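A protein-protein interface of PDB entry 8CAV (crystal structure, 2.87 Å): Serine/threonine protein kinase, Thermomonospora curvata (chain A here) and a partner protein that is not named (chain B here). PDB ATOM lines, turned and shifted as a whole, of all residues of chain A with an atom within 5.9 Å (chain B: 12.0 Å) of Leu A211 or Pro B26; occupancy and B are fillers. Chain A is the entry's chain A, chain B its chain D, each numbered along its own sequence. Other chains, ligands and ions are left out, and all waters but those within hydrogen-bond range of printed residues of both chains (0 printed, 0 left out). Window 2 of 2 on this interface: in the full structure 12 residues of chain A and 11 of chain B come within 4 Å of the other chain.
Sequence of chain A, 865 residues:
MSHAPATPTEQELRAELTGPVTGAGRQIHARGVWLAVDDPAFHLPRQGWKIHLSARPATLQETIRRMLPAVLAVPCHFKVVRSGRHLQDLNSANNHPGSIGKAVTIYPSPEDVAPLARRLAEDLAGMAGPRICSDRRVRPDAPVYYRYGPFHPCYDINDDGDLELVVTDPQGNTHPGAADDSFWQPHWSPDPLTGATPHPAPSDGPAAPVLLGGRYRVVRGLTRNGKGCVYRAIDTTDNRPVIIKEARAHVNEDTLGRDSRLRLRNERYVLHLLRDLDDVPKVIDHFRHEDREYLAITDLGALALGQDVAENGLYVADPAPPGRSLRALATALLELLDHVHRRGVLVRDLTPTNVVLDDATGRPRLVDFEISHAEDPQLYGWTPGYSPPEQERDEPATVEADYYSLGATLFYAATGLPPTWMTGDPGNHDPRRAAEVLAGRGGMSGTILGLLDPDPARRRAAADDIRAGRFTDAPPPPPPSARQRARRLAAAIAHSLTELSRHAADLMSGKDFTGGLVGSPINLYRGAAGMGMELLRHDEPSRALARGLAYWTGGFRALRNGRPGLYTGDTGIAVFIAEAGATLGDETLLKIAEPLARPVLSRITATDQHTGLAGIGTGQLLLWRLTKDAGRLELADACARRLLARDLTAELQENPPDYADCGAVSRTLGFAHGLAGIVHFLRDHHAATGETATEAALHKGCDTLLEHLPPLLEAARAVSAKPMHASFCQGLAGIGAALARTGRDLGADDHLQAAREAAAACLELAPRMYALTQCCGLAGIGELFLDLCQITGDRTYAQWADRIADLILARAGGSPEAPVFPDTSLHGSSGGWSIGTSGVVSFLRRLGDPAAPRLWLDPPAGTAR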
ATOM      1  N   PRO A 209     -28.791 -13.728 -18.965  1.00  0.00           N
ATOM      2  CA  PRO A 209     -27.705 -14.048 -18.029  1.00  0.00           C
ATOM      3  C   PRO A 209     -27.971 -13.499 -16.634  1.00  0.00           C
ATOM      4  O   PRO A 209     -28.513 -12.404 -16.469  1.00  0.00           O
ATOM      5  CB  PRO A 209     -26.473 -13.389 -18.667  1.00  0.00           C
ATOM      6  CG  PRO A 209     -27.020 -12.373 -19.622  1.00  0.00           C
ATOM      7  CD  PRO A 209     -28.314 -12.941 -20.117  1.00  0.00           C
ATOM      8  N   VAL A 210     -27.571 -14.271 -15.623  1.00  0.00           N
ATOM      9  CA  VAL A 210     -27.788 -13.927 -14.222  1.00  0.00           C
ATOM     10  C   VAL A 210     -26.440 -13.593 -13.594  1.00  0.00           C
ATOM     11  O   VAL A 210     -25.550 -14.448 -13.513  1.00  0.00           O
ATOM     12  CB  VAL A 210     -28.507 -15.053 -13.455  1.00  0.00           C
ATOM     13  CG1 VAL A 210     -28.461 -16.369 -14.228  1.00  0.00           C
ATOM     14  CG2 VAL A 210     -27.923 -15.234 -12.047  1.00  0.00           C
ATOM     15  N   LEU A 211     -26.298 -12.343 -13.157  1.00  0.00           N
ATOM     16  CA  LEU A 211     -25.125 -11.850 -12.450  1.00  0.00           C
ATOM     17  C   LEU A 211     -25.618 -10.977 -11.308  1.00  0.00           C
ATOM     18  O   LEU A 211     -26.505 -10.142 -11.504  1.00  0.00           O
ATOM     19  CB  LEU A 211     -24.204 -11.045 -13.377  1.00  0.00           C
ATOM     20  CG  LEU A 211     -23.769  -9.645 -12.930  1.00  0.00           C
ATOM     21  CD1 LEU A 211     -22.581  -9.718 -11.976  1.00  0.00           C
ATOM     22  CD2 LEU A 211     -23.447  -8.768 -14.136  1.00  0.00           C
ATOM     23  N   LEU A 212     -25.033 -11.147 -10.125  1.00  0.00           N
ATOM     24  CA  LEU A 212     -25.456 -10.353  -8.982  1.00  0.00           C
ATOM     25  C   LEU A 212     -24.303 -10.183  -8.007  1.00  0.00           C
ATOM     26  O   LEU A 212     -23.333 -10.947  -8.010  1.00  0.00           O
ATOM     27  CB  LEU A 212     -26.662 -10.987  -8.278  1.00  0.00           C
ATOM     28  CG  LEU A 212     -27.987 -10.876  -9.038  1.00  0.00           C
ATOM     29  CD1 LEU A 212     -29.076 -11.696  -8.368  1.00  0.00           C
ATOM     30  CD2 LEU A 212     -28.410  -9.415  -9.155  1.00  0.00           C
ATOM     31  N   GLY A 213     -24.427  -9.157  -7.167  1.00  0.00           N
ATOM     32  CA  GLY A 213     -23.435  -8.868  -6.158  1.00  0.00           C
ATOM     33  C   GLY A 213     -23.624  -9.700  -4.905  1.00  0.00           C
ATOM     34  O   GLY A 213     -24.506 -10.553  -4.803  1.00  0.00           O
ATOM     35  N   VAL A 219     -22.156  -4.962  -8.781  1.00  0.00           N
ATOM     36  CA  VAL A 219     -20.887  -4.755  -9.481  1.00  0.00           C
ATOM     37  C   VAL A 219     -21.111  -4.393 -10.957  1.00  0.00           C
ATOM     38  O   VAL A 219     -22.226  -4.444 -11.476  1.00  0.00           O
ATOM     39  CB  VAL A 219     -19.961  -5.989  -9.373  1.00  0.00           C
ATOM     40  CG1 VAL A 219     -20.118  -6.652  -8.010  1.00  0.00           C
ATOM     41  CG2 VAL A 219     -20.234  -6.981 -10.501  1.00  0.00           C
ATOM     42  N   ARG A 220     -20.000  -4.030 -11.630  1.00  0.00           N
ATOM     43  CA  ARG A 220     -20.004  -3.596 -13.027  1.00  0.00           C
ATOM     44  C   ARG A 220     -18.605  -3.612 -13.666  1.00  0.00           C
ATOM     45  O   ARG A 220     -18.092  -2.562 -14.067  1.00  0.00           O
ATOM     46  CB  ARG A 220     -20.603  -2.181 -13.129  1.00  0.00           C
ATOM     47  CG  ARG A 220     -21.636  -1.954 -14.245  1.00  0.00           C
ATOM     48  CD  ARG A 220     -21.116  -2.344 -15.623  1.00  0.00           C
ATOM     49  NE  ARG A 220     -22.045  -1.984 -16.691  1.00  0.00           N
ATOM     50  CZ  ARG A 220     -23.181  -2.621 -16.946  1.00  0.00           C
ATOM     51  NH1 ARG A 220     -23.590  -3.633 -16.197  1.00  0.00           N
ATOM     52  NH2 ARG A 220     -23.928  -2.233 -17.977  1.00  0.00           N
ATOM     53  N   GLY A 221     -17.977  -4.784 -13.781  1.00  0.00           N
ATOM     54  CA  GLY A 221     -16.736  -4.926 -14.558  1.00  0.00           C
ATOM     55  C   GLY A 221     -15.577  -4.081 -14.037  1.00  0.00           C
ATOM     56  O   GLY A 221     -15.386  -3.935 -12.839  1.00  0.00           O
ATOM     57  N   LEU A 222     -14.737  -3.603 -14.975  1.00  0.00           N
ATOM     58  CA  LEU A 222     -13.772  -2.510 -14.820  1.00  0.00           C
ATOM     59  C   LEU A 222     -12.285  -2.881 -14.930  1.00  0.00           C
ATOM     60  O   LEU A 222     -11.451  -1.974 -15.023  1.00  0.00           O
ATOM     61  CB  LEU A 222     -13.964  -1.763 -13.478  1.00  0.00           C
ATOM     62  CG  LEU A 222     -13.308  -0.372 -13.429  1.00  0.00           C
ATOM     63  CD1 LEU A 222     -13.693   0.469 -14.651  1.00  0.00           C
ATOM     64  CD2 LEU A 222     -13.656   0.396 -12.158  1.00  0.00           C
ATOM     65  N   ALA B  20     -20.496 -16.402  -0.603  1.00  0.00           N
ATOM     66  CA  ALA B  20     -20.246 -15.675  -1.836  1.00  0.00           C
ATOM     67  C   ALA B  20     -21.066 -16.246  -2.982  1.00  0.00           C
ATOM     68  O   ALA B  20     -21.148 -17.463  -3.158  1.00  0.00           O
ATOM     69  CB  ALA B  20     -18.761 -15.718  -2.210  1.00  0.00           C
ATOM     70  N   ILE B  21     -21.653 -15.348  -3.770  1.00  0.00           N
ATOM     71  CA  ILE B  21     -22.435 -15.696  -4.942  1.00  0.00           C
ATOM     72  C   ILE B  21     -21.630 -15.598  -6.229  1.00  0.00           C
ATOM     73  O   ILE B  21     -22.199 -15.742  -7.319  1.00  0.00           O
ATOM     74  CB  ILE B  21     -23.666 -14.787  -5.027  1.00  0.00           C
ATOM     75  N   LYS B  22     -20.322 -15.358  -6.130  1.00  0.00           N
ATOM     76  CA  LYS B  22     -19.506 -15.095  -7.308  1.00  0.00           C
ATOM     77  C   LYS B  22     -19.633 -16.231  -8.312  1.00  0.00           C
ATOM     78  O   LYS B  22     -19.479 -17.403  -7.963  1.00  0.00           O
ATOM     79  CB  LYS B  22     -18.040 -14.913  -6.903  1.00  0.00           C
ATOM     80  N   TRP B  23     -19.912 -15.874  -9.568  1.00  0.00           N
ATOM     81  CA  TRP B  23     -20.112 -16.865 -10.614  1.00  0.00           C
ATOM     82  C   TRP B  23     -19.260 -16.579 -11.844  1.00  0.00           C
ATOM     83  O   TRP B  23     -18.394 -17.387 -12.194  1.00  0.00           O
ATOM     84  CB  TRP B  23     -21.596 -16.931 -10.996  1.00  0.00           C
ATOM     85  N   GLU B  24     -19.475 -15.438 -12.508  1.00  0.00           N
ATOM     86  CA  GLU B  24     -18.819 -15.173 -13.778  1.00  0.00           C
ATOM     87  C   GLU B  24     -18.426 -13.708 -13.910  1.00  0.00           C
ATOM     88  O   GLU B  24     -18.752 -12.867 -13.066  1.00  0.00           O
ATOM     89  CB  GLU B  24     -19.722 -15.567 -14.960  1.00  0.00           C
ATOM     90  N   ALA B  25     -17.717 -13.417 -15.002  1.00  0.00           N
ATOM     91  CA  ALA B  25     -17.263 -12.069 -15.312  1.00  0.00           C
ATOM     92  C   ALA B  25     -18.414 -11.198 -15.803  1.00  0.00           C
ATOM     93  O   ALA B  25     -19.386 -11.683 -16.388  1.00  0.00           O
ATOM     94  CB  ALA B  25     -16.166 -12.126 -16.381  1.00  0.00           C
ATOM     95  N   PRO B  26     -18.284  -9.889 -15.575  1.00  0.00           N
ATOM     96  CA  PRO B  26     -19.320  -8.917 -15.896  1.00  0.00           C
ATOM     97  C   PRO B  26     -18.722  -7.730 -16.642  1.00  0.00           C
ATOM     98  O   PRO B  26     -17.520  -7.472 -16.576  1.00  0.00           O
ATOM     99  CB  PRO B  26     -20.027  -8.432 -14.621  1.00  0.00           C
ATOM    100  N   ALA B  27     -19.588  -7.011 -17.368  1.00  0.00           N
ATOM    101  CA  ALA B  27     -19.245  -5.767 -18.053  1.00  0.00           C
ATOM    102  C   ALA B  27     -18.087  -5.902 -19.037  1.00  0.00           C
ATOM    103  O   ALA B  27     -17.653  -7.018 -19.339  1.00  0.00           O
ATOM    104  CB  ALA B  27     -18.921  -4.676 -17.025  1.00  0.00           C
ATOM    105  N   HIS B  28     -17.596  -4.767 -19.565  1.00  0.00           N
ATOM    106  CA  HIS B  28     -16.481  -4.751 -20.514  1.00  0.00           C
ATOM    107  C   HIS B  28     -15.766  -3.396 -20.458  1.00  0.00           C
ATOM    108  O   HIS B  28     -15.855  -2.572 -21.366  1.00  0.00           O
ATOM    109  CB  HIS B  28     -16.955  -5.045 -21.940  1.00  0.00           C
ATOM    110  N   GLN B  29     -15.023  -3.167 -19.376  1.00  0.00           N
ATOM    111  CA  GLN B  29     -14.214  -1.959 -19.242  1.00  0.00           C
ATOM    112  C   GLN B  29     -12.787  -2.315 -18.836  1.00  0.00           C
ATOM    113  O   GLN B  29     -11.831  -1.931 -19.506  1.00  0.00           O
ATOM    114  CB  GLN B  29     -14.829  -1.008 -18.229  1.00  0.00           C
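Among the printed residues, merely in contact across the chains: Leu A211 with Pro B26, Arg A220 with Ala B27, Gly A221 with Pro B26, Gly A221 with Ala B27 and Leu A222 with Gln B29.
No residue of chain B comes within 4 Å of Pro A209. Val A210 touches none of the printed residues of chain B. Leu A211 touches just one residue of chain B: Pro B26 (3.5 Å). Leu A212 touches none of the printed residues of chain B. No residue of chain B comes within 4 Å of Val A219. Of the printed residues of chain B, Leu A222 touches Gln B29. Ile B21 touches none of the printed residues of chain A. Pro B26 touches just these residues of chain A: Leu A211 (3.5 Å) and Gly A221 (3.3 Å). Printed residues of chain A within 4 Å of Ala B27: Arg A220 and Gly A221. Of the printed residues of chain A, Gln B29 touches Leu A222 (3.9 Å). The nearest residue of chain B that does not touch Leu A211 is Glu B24 (5.1 Å). The nearest residue of chain A that does not touch Pro B26 is Val A219 (4.4 Å). The nearest printed residue of chain A that does not touch Ala B27 is Leu A222 (4.8 Å).
Printed residues of chain B that touch a printed residue of chain A: Pro B26, Ala B27 and Gln B29. Hydrophobic or aromatic side chains of chain B within 4 Å of the printed part of chain A: Pro B26 and Ala B27. Of the 9 printed residues of chain A, 4 touch a printed residue of chain B. Hydrophobic or aromatic side chains of chain A that line the printed part of chain B: Leu A211. Among the printed residues, 5 pairs touch across the chains. Among the printed residues, no Asp or Glu carboxylate lies within 4 Å of a Lys or Arg side-chain nitrogen of the other chain.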
